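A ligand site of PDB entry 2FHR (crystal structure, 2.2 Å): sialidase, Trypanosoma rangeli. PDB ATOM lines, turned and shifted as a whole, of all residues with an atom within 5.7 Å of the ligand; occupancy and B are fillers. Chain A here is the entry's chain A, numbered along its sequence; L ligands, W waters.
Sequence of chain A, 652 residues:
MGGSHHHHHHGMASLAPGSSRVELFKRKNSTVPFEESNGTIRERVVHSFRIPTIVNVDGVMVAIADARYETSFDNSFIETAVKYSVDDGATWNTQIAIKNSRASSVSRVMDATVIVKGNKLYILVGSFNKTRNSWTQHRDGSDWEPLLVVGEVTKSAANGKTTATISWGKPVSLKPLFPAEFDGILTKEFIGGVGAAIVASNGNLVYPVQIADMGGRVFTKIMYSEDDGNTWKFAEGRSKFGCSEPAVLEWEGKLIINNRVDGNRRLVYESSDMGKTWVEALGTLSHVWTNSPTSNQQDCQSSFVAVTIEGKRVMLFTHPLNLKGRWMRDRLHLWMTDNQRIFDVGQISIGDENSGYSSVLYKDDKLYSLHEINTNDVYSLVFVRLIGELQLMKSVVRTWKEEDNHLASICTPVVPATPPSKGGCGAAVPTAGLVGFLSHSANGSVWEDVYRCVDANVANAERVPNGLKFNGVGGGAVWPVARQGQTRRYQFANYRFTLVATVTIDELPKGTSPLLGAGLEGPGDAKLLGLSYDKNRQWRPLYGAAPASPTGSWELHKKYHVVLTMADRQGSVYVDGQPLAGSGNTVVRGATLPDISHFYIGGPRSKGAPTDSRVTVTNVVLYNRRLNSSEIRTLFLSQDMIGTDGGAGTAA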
ATOM      1  N   ARG A  50     -12.257   9.878   7.050  1.00  0.00           N
ATOM      2  CA  ARG A  50     -12.121   8.426   7.183  1.00  0.00           C
ATOM      3  C   ARG A  50     -11.496   7.782   5.972  1.00  0.00           C
ATOM      4  O   ARG A  50     -11.351   8.395   4.939  1.00  0.00           O
ATOM      5  CB  ARG A  50     -13.492   7.770   7.530  1.00  0.00           C
ATOM      6  CG  ARG A  50     -13.866   8.019   8.982  1.00  0.00           C
ATOM      7  CD  ARG A  50     -14.717   6.981   9.528  1.00  0.00           C
ATOM      8  NE  ARG A  50     -13.943   5.783   9.587  1.00  0.00           N
ATOM      9  CZ  ARG A  50     -14.415   4.555   9.588  1.00  0.00           C
ATOM     10  NH1 ARG A  50     -13.570   3.539   9.629  1.00  0.00           N
ATOM     11  NH2 ARG A  50     -15.721   4.339   9.613  1.00  0.00           N
ATOM     12  N   ILE A  51     -11.086   6.539   6.139  1.00  0.00           N
ATOM     13  CA  ILE A  51     -10.712   5.665   5.022  1.00  0.00           C
ATOM     14  C   ILE A  51      -9.531   6.229   4.193  1.00  0.00           C
ATOM     15  O   ILE A  51      -9.667   6.384   2.917  1.00  0.00           O
ATOM     16  CB  ILE A  51     -11.930   5.381   4.047  1.00  0.00           C
ATOM     17  CG1 ILE A  51     -13.242   5.287   4.785  1.00  0.00           C
ATOM     18  CG2 ILE A  51     -11.689   4.119   3.205  1.00  0.00           C
ATOM     19  CD1 ILE A  51     -13.306   4.264   5.888  1.00  0.00           C
ATOM     20  N   ASP A  66     -12.257   9.766   2.558  1.00  0.00           N
ATOM     21  CA  ASP A  66     -13.651  10.095   2.606  1.00  0.00           C
ATOM     22  C   ASP A  66     -13.711  11.414   3.369  1.00  0.00           C
ATOM     23  O   ASP A  66     -13.163  11.515   4.467  1.00  0.00           O
ATOM     24  CB  ASP A  66     -14.477   9.143   3.458  1.00  0.00           C
ATOM     25  CG  ASP A  66     -14.939   7.872   2.752  1.00  0.00           C
ATOM     26  OD1 ASP A  66     -14.392   7.470   1.696  1.00  0.00           O
ATOM     27  OD2 ASP A  66     -15.847   7.238   3.341  1.00  0.00           O
ATOM     28  N   ARG A  68     -16.540  12.910   5.105  1.00  0.00           N
ATOM     29  CA  ARG A  68     -17.861  12.617   5.633  1.00  0.00           C
ATOM     30  C   ARG A  68     -18.369  13.952   6.228  1.00  0.00           C
ATOM     31  O   ARG A  68     -18.062  14.356   7.374  1.00  0.00           O
ATOM     32  CB  ARG A  68     -17.800  11.410   6.630  1.00  0.00           C
ATOM     33  CG  ARG A  68     -17.290  10.104   5.939  1.00  0.00           C
ATOM     34  CD  ARG A  68     -17.428   8.796   6.743  1.00  0.00           C
ATOM     35  NE  ARG A  68     -16.972   7.641   5.951  1.00  0.00           N
ATOM     36  CZ  ARG A  68     -17.237   6.361   6.207  1.00  0.00           C
ATOM     37  NH1 ARG A  68     -17.934   5.992   7.289  1.00  0.00           N
ATOM     38  NH2 ARG A  68     -16.792   5.412   5.414  1.00  0.00           N
ATOM     39  N   ASP A  74     -21.490   5.525   7.807  1.00  0.00           N
ATOM     40  CA  ASP A  74     -21.222   5.043   6.449  1.00  0.00           C
ATOM     41  C   ASP A  74     -22.263   5.553   5.447  1.00  0.00           C
ATOM     42  O   ASP A  74     -21.918   5.982   4.343  1.00  0.00           O
ATOM     43  CB  ASP A  74     -21.231   3.469   6.374  1.00  0.00           C
ATOM     44  CG  ASP A  74     -20.167   2.784   7.251  1.00  0.00           C
ATOM     45  OD1 ASP A  74     -20.311   1.533   7.502  1.00  0.00           O
ATOM     46  OD2 ASP A  74     -19.207   3.456   7.716  1.00  0.00           O
ATOM     47  N   ASN A  75     -23.546   5.508   5.791  1.00  0.00           N
ATOM     48  CA  ASN A  75     -24.561   5.795   4.772  1.00  0.00           C
ATOM     49  C   ASN A  75     -25.093   7.245   4.875  1.00  0.00           C
ATOM     50  O   ASN A  75     -26.264   7.469   5.146  1.00  0.00           O
ATOM     51  CB  ASN A  75     -25.643   4.732   4.832  1.00  0.00           C
ATOM     52  CG  ASN A  75     -25.056   3.323   4.940  1.00  0.00           C
ATOM     53  OD1 ASN A  75     -24.256   2.900   4.082  1.00  0.00           O
ATOM     54  ND2 ASN A  75     -25.407   2.611   6.007  1.00  0.00           N
ATOM     55  N   MET A 110     -17.258   6.592  -1.773  1.00  0.00           N
ATOM     56  CA  MET A 110     -16.565   6.147  -0.596  1.00  0.00           C
ATOM     57  C   MET A 110     -15.668   4.923  -0.837  1.00  0.00           C
ATOM     58  O   MET A 110     -15.813   4.197  -1.813  1.00  0.00           O
ATOM     59  CB  MET A 110     -17.639   5.834   0.479  1.00  0.00           C
ATOM     60  CG  MET A 110     -18.465   4.615   0.185  1.00  0.00           C
ATOM     61  SD  MET A 110     -19.926   4.508   1.225  1.00  0.00           S
ATOM     62  CE  MET A 110     -19.278   4.322   2.857  1.00  0.00           C
ATOM     63  N   ASP A 111     -14.695   4.757   0.039  1.00  0.00           N
ATOM     64  CA  ASP A 111     -13.934   3.553   0.161  1.00  0.00           C
ATOM     65  C   ASP A 111     -12.974   3.347  -1.026  1.00  0.00           C
ATOM     66  O   ASP A 111     -12.882   2.225  -1.606  1.00  0.00           O
ATOM     67  CB  ASP A 111     -14.876   2.341   0.330  1.00  0.00           C
ATOM     68  CG  ASP A 111     -15.374   2.181   1.782  1.00  0.00           C
ATOM     69  OD1 ASP A 111     -15.272   3.145   2.578  1.00  0.00           O
ATOM     70  OD2 ASP A 111     -15.852   1.036   2.080  1.00  0.00           O
ATOM     71  N   PHE A 128     -23.187   5.578  -4.197  1.00  0.00           N
ATOM     72  CA  PHE A 128     -24.549   5.217  -3.771  1.00  0.00           C
ATOM     73  C   PHE A 128     -25.382   6.496  -3.765  1.00  0.00           C
ATOM     74  O   PHE A 128     -24.850   7.579  -3.564  1.00  0.00           O
ATOM     75  CB  PHE A 128     -24.544   4.558  -2.370  1.00  0.00           C
ATOM     76  CG  PHE A 128     -23.705   3.316  -2.291  1.00  0.00           C
ATOM     77  CD1 PHE A 128     -22.343   3.399  -2.079  1.00  0.00           C
ATOM     78  CD2 PHE A 128     -24.279   2.053  -2.447  1.00  0.00           C
ATOM     79  CE1 PHE A 128     -21.575   2.192  -1.997  1.00  0.00           C
ATOM     80  CE2 PHE A 128     -23.551   0.912  -2.368  1.00  0.00           C
ATOM     81  CZ  PHE A 128     -22.189   0.959  -2.153  1.00  0.00           C
ATOM     82  N   SER A 134     -26.778  -0.781   4.806  1.00  0.00           N
ATOM     83  CA  SER A 134     -25.462  -1.242   4.502  1.00  0.00           C
ATOM     84  C   SER A 134     -25.394  -2.023   3.183  1.00  0.00           C
ATOM     85  O   SER A 134     -26.286  -2.811   2.846  1.00  0.00           O
ATOM     86  CB  SER A 134     -24.943  -2.031   5.705  1.00  0.00           C
ATOM     87  OG  SER A 134     -23.614  -2.435   5.506  1.00  0.00           O
ATOM     88  N   TRP A 135     -24.334  -1.801   2.425  1.00  0.00           N
ATOM     89  CA  TRP A 135     -24.267  -2.306   1.043  1.00  0.00           C
ATOM     90  C   TRP A 135     -24.516  -3.813   0.937  1.00  0.00           C
ATOM     91  O   TRP A 135     -25.262  -4.258   0.096  1.00  0.00           O
ATOM     92  CB  TRP A 135     -22.932  -1.871   0.365  1.00  0.00           C
ATOM     93  CG  TRP A 135     -21.684  -2.598   0.794  1.00  0.00           C
ATOM     94  CD1 TRP A 135     -21.007  -2.440   2.000  1.00  0.00           C
ATOM     95  CD2 TRP A 135     -20.903  -3.537   0.023  1.00  0.00           C
ATOM     96  NE1 TRP A 135     -19.883  -3.226   1.990  1.00  0.00           N
ATOM     97  CE2 TRP A 135     -19.822  -3.941   0.816  1.00  0.00           C
ATOM     98  CE3 TRP A 135     -21.035  -4.082  -1.245  1.00  0.00           C
ATOM     99  CZ2 TRP A 135     -18.881  -4.871   0.366  1.00  0.00           C
ATOM    100  CZ3 TRP A 135     -20.129  -5.018  -1.669  1.00  0.00           C
ATOM    101  CH2 TRP A 135     -19.021  -5.377  -0.864  1.00  0.00           C
ATOM    102  N   THR A 136     -23.946  -4.587   1.832  1.00  0.00           N
ATOM    103  CA  THR A 136     -24.144  -6.038   1.817  1.00  0.00           C
ATOM    104  C   THR A 136     -25.587  -6.428   2.031  1.00  0.00           C
ATOM    105  O   THR A 136     -25.958  -7.561   1.705  1.00  0.00           O
ATOM    106  CB  THR A 136     -23.284  -6.748   2.892  1.00  0.00           C
ATOM    107  OG1 THR A 136     -23.681  -6.314   4.218  1.00  0.00           O
ATOM    108  CG2 THR A 136     -21.769  -6.445   2.630  1.00  0.00           C
ATOM    109  N   ILE A 191     -16.994  -3.541  -4.422  1.00  0.00           N
ATOM    110  CA  ILE A 191     -16.195  -2.348  -4.295  1.00  0.00           C
ATOM    111  C   ILE A 191     -14.743  -2.764  -4.236  1.00  0.00           C
ATOM    112  O   ILE A 191     -14.440  -3.961  -4.178  1.00  0.00           O
ATOM    113  CB  ILE A 191     -16.649  -1.468  -3.085  1.00  0.00           C
ATOM    114  CG1 ILE A 191     -17.007  -2.306  -1.879  1.00  0.00           C
ATOM    115  CG2 ILE A 191     -17.909  -0.743  -3.422  1.00  0.00           C
ATOM    116  CD1 ILE A 191     -17.918  -1.539  -0.848  1.00  0.00           C
ATOM    117  N   GLN A 210     -14.005  -6.623  -3.268  1.00  0.00           N
ATOM    118  CA  GLN A 210     -14.920  -7.230  -2.392  1.00  0.00           C
ATOM    119  C   GLN A 210     -16.298  -7.265  -3.055  1.00  0.00           C
ATOM    120  O   GLN A 210     -16.764  -6.257  -3.590  1.00  0.00           O
ATOM    121  CB  GLN A 210     -14.904  -6.566  -0.996  1.00  0.00           C
ATOM    122  CG  GLN A 210     -15.213  -5.091  -0.972  1.00  0.00           C
ATOM    123  CD  GLN A 210     -14.968  -4.423   0.356  1.00  0.00           C
ATOM    124  OE1 GLN A 210     -14.383  -3.320   0.400  1.00  0.00           O
ATOM    125  NE2 GLN A 210     -15.378  -5.056   1.425  1.00  0.00           N
ATOM    126  N   SER A 244     -13.525  -9.774   3.393  1.00  0.00           N
ATOM    127  CA  SER A 244     -13.804  -8.415   2.939  1.00  0.00           C
ATOM    128  C   SER A 244     -12.517  -7.606   2.884  1.00  0.00           C
ATOM    129  O   SER A 244     -11.432  -8.120   3.167  1.00  0.00           O
ATOM    130  CB  SER A 244     -14.785  -7.708   3.901  1.00  0.00           C
ATOM    131  OG  SER A 244     -14.445  -7.831   5.259  1.00  0.00           O
ATOM    132  N   GLU A 245     -12.686  -6.368   2.415  1.00  0.00           N
ATOM    133  CA  GLU A 245     -11.671  -5.342   2.265  1.00  0.00           C
ATOM    134  C   GLU A 245     -10.284  -5.956   2.011  1.00  0.00           C
ATOM    135  O   GLU A 245      -9.404  -5.875   2.872  1.00  0.00           O
ATOM    136  CB  GLU A 245     -11.662  -4.460   3.517  1.00  0.00           C
ATOM    137  CG  GLU A 245     -12.855  -3.579   3.571  1.00  0.00           C
ATOM    138  CD  GLU A 245     -12.858  -2.607   4.738  1.00  0.00           C
ATOM    139  OE1 GLU A 245     -12.171  -2.884   5.773  1.00  0.00           O
ATOM    140  OE2 GLU A 245     -13.493  -1.526   4.568  1.00  0.00           O
ATOM    141  N   ARG A 260      -9.706  -8.935   5.364  1.00  0.00           N
ATOM    142  CA  ARG A 260     -10.480  -8.655   6.526  1.00  0.00           C
ATOM    143  C   ARG A 260     -11.441  -9.817   6.761  1.00  0.00           C
ATOM    144  O   ARG A 260     -11.937 -10.353   5.815  1.00  0.00           O
ATOM    145  CB  ARG A 260     -11.256  -7.333   6.337  1.00  0.00           C
ATOM    146  CG  ARG A 260     -12.058  -7.026   7.563  1.00  0.00           C
ATOM    147  CD  ARG A 260     -12.701  -5.665   7.539  1.00  0.00           C
ATOM    148  NE  ARG A 260     -13.876  -5.609   8.400  1.00  0.00           N
ATOM    149  CZ  ARG A 260     -14.534  -4.500   8.737  1.00  0.00           C
ATOM    150  NH1 ARG A 260     -14.150  -3.323   8.254  1.00  0.00           N
ATOM    151  NH2 ARG A 260     -15.630  -4.552   9.542  1.00  0.00           N
ATOM    152  N   ASP A 262     -14.413 -10.353   9.493  1.00  0.00           N
ATOM    153  CA  ASP A 262     -15.126 -10.065  10.754  1.00  0.00           C
ATOM    154  C   ASP A 262     -15.364 -11.377  11.538  1.00  0.00           C
ATOM    155  O   ASP A 262     -15.767 -12.390  10.993  1.00  0.00           O
ATOM    156  CB  ASP A 262     -16.451  -9.379  10.449  1.00  0.00           C
ATOM    157  CG  ASP A 262     -16.242  -8.052   9.791  1.00  0.00           C
ATOM    158  OD1 ASP A 262     -16.958  -7.712   8.818  1.00  0.00           O
ATOM    159  OD2 ASP A 262     -15.333  -7.357  10.237  1.00  0.00           O
ATOM    160  N   ASP A 299     -13.666  -7.041  12.494  1.00  0.00           N
ATOM    161  CA  ASP A 299     -12.308  -6.866  12.068  1.00  0.00           C
ATOM    162  C   ASP A 299     -12.189  -5.452  11.528  1.00  0.00           C
ATOM    163  O   ASP A 299     -13.105  -4.637  11.661  1.00  0.00           O
ATOM    164  CB  ASP A 299     -11.927  -7.948  11.050  1.00  0.00           C
ATOM    165  CG  ASP A 299     -10.429  -8.076  10.789  1.00  0.00           C
ATOM    166  OD1 ASP A 299      -9.632  -7.321  11.394  1.00  0.00           O
ATOM    167  OD2 ASP A 299     -10.056  -8.898   9.903  1.00  0.00           O
ATOM    168  N   ARG A 329     -10.805  -0.143  17.991  1.00  0.00           N
ATOM    169  CA  ARG A 329      -9.601  -0.307  17.181  1.00  0.00           C
ATOM    170  C   ARG A 329      -8.415   0.521  17.724  1.00  0.00           C
ATOM    171  O   ARG A 329      -7.702   1.243  16.989  1.00  0.00           O
ATOM    172  CB  ARG A 329      -9.918   0.075  15.748  1.00  0.00           C
ATOM    173  CG  ARG A 329     -10.898  -0.876  15.077  1.00  0.00           C
ATOM    174  CD  ARG A 329     -11.534  -0.194  13.878  1.00  0.00           C
ATOM    175  NE  ARG A 329     -12.401  -1.148  13.244  1.00  0.00           N
ATOM    176  CZ  ARG A 329     -13.309  -0.871  12.331  1.00  0.00           C
ATOM    177  NH1 ARG A 329     -13.457   0.346  11.886  1.00  0.00           N
ATOM    178  NH2 ARG A 329     -14.027  -1.859  11.816  1.00  0.00           N
ATOM    179  N   TYR A 357      -8.754   2.549  10.394  1.00  0.00           N
ATOM    180  CA  TYR A 357      -8.210   2.311   9.067  1.00  0.00           C
ATOM    181  C   TYR A 357      -6.925   3.071   8.909  1.00  0.00           C
ATOM    182  O   TYR A 357      -6.775   4.124   9.455  1.00  0.00           O
ATOM    183  CB  TYR A 357      -9.195   2.715   7.974  1.00  0.00           C
ATOM    184  CG  TYR A 357     -10.455   1.837   7.769  1.00  0.00           C
ATOM    185  CD1 TYR A 357     -11.019   1.040   8.783  1.00  0.00           C
ATOM    186  CD2 TYR A 357     -11.062   1.818   6.534  1.00  0.00           C
ATOM    187  CE1 TYR A 357     -12.205   0.243   8.562  1.00  0.00           C
ATOM    188  CE2 TYR A 357     -12.231   1.040   6.293  1.00  0.00           C
ATOM    189  CZ  TYR A 357     -12.821   0.269   7.290  1.00  0.00           C
ATOM    190  OH  TYR A 357     -14.013  -0.391   6.958  1.00  0.00           O
HETATM  191  C1  LIG L   1     -15.400   0.063   8.977  1.00  0.00           C
HETATM  192  F1  LIG L   1     -16.613   1.984   7.685  1.00  0.00           F
HETATM  193  C2  LIG L   1     -15.266   0.072   7.436  1.00  0.00           C
HETATM  194  C3  LIG L   1     -15.592   1.479   6.941  1.00  0.00           C
HETATM  195  C4  LIG L   1     -15.997   1.404   5.456  1.00  0.00           C
HETATM  196  O1  LIG L   1     -16.168   2.723   4.954  1.00  0.00           O
HETATM  197  C5  LIG L   1     -17.325   0.590   5.327  1.00  0.00           C
HETATM  198  N1  LIG L   1     -17.874   0.706   4.108  1.00  0.00           N
HETATM  199  C6  LIG L   1     -16.979  -0.827   5.799  1.00  0.00           C
HETATM  200  O2  LIG L   1     -16.441  -0.776   7.159  1.00  0.00           O
HETATM  201  C7  LIG L   1     -18.196  -1.784   5.765  1.00  0.00           C
HETATM  202  O3  LIG L   1     -19.258  -1.297   6.574  1.00  0.00           O
HETATM  203  C8  LIG L   1     -17.909  -3.171   6.305  1.00  0.00           C
HETATM  204  O4  LIG L   1     -16.803  -3.778   5.623  1.00  0.00           O
HETATM  205  C9  LIG L   1     -19.205  -4.009   6.264  1.00  0.00           C
HETATM  206  O5  LIG L   1     -19.403  -4.634   5.002  1.00  0.00           O
HETATM  207  C10 LIG L   1     -19.107   0.487   3.644  1.00  0.00           C
HETATM  208  O6  LIG L   1     -20.077   0.075   4.323  1.00  0.00           O
HETATM  209  C11 LIG L   1     -19.294   0.718   2.144  1.00  0.00           C
HETATM  210  O7  LIG L   1     -15.622  -1.059   9.466  1.00  0.00           O
HETATM  211  O8  LIG L   1     -15.307   1.094   9.732  1.00  0.00           O
HETATM  212  O   HOH W   1     -19.085  -0.266   9.003  1.00  0.00           O
HETATM  213  O   HOH W   2     -16.952   1.325  11.914  1.00  0.00           O
HETATM  214  O   HOH W   3     -22.471   0.743   3.346  1.00  0.00           O
HETATM  215  O   HOH W   4     -16.782  -3.443   3.126  1.00  0.00           O
HETATM  216  O   HOH W   5     -22.230  -4.421   4.707  1.00  0.00           O
HETATM  217  O   HOH W   6     -16.329  -6.306   6.432  1.00  0.00           O
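The guanidinium group (NH1) of Arg 260 is in hydrogen-bond range of the side-chain hydroxyl (OH) of Tyr 357, at 3.2 Å. OH of Tyr 357 lies close to OE2 of Glu 245, at 2.7 Å. The backbone NH (N) of Asp 111 is in hydrogen-bond range of the side-chain carboxylate (OD1) of Asp 66, 3.2 Å away. The guanidinium group (NH1) of Arg 68 is in salt-bridge range of the side-chain carboxylate (OD2) of Asp 74 (2.9 Å). The guanidinium group of Arg 260 lies close to the backbone carbonyl oxygen of Asp 299 (3.3 Å). OD2 of Asp 262 lies within salt-bridge range of NH2 of Arg 260. N of Asp 66 lies within hydrogen-bond range of O of Arg 50 (2.9 Å). The backbone carbonyl oxygen of Ile 191 sits at hydrogen-bond distance from the backbone NH of Gln 210 (2.8 Å).
Merely in contact with the ligand: Ile 51 (3.4 Å), Met 110 (3.7 Å), Glu 245 (3.7 Å), Thr 136 (3.8 Å) and Ile 191 (3.99 Å).
OH of Tyr 357 is covalently linked to C2 of the ligand, 1.4 Å away. OD1 of Asp 111 sits at hydrogen-bond distance from O1 of the ligand, 2.6 Å away. The guanidinium group (NH2) of Arg 68 lies within hydrogen-bond range of an oxygen (O1) of the ligand (2.8 Å). An oxygen (O8) of the ligand lies within salt-bridge range of the guanidinium group (NH1) of Arg 329 (2.9 Å). An oxygen (O7) of the ligand lies within salt-bridge range of the guanidinium group (NH1) of Arg 260, at 3.0 Å. OD1 of Asp 74 sits at hydrogen-bond distance from O3 of the ligand (3.2 Å). NH1 of Arg 50 is in salt-bridge range of O8 of the ligand, 3.0 Å away. An oxygen (O5) of the ligand is in hydrogen-bond range of the indole nitrogen of Trp 135, 3.4 Å away.
Water W4 lies within hydrogen-bond range of O4 of the ligand (2.5 Å), NE2 of Gln 210 (2.7 Å) and NE1 of Trp 135 (3.3 Å). Water W1 lies within hydrogen-bond range of O3 of the ligand (2.6 Å) and OD1 of Asp 74 (2.6 Å). Water W3 lies within hydrogen-bond range of O6 of the ligand, OD1 of Asn 75 and N of Trp 135. Water W6 lies within hydrogen-bond range of OG of Ser 244 (2.7 Å), O4 of the ligand (2.7 Å), OD1 of Asp 262 (2.8 Å) and NE of Arg 260 (3.2 Å). Water W5 lies within hydrogen-bond range of OG1 of Thr 136, OG of Ser 134 and O5 of the ligand.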
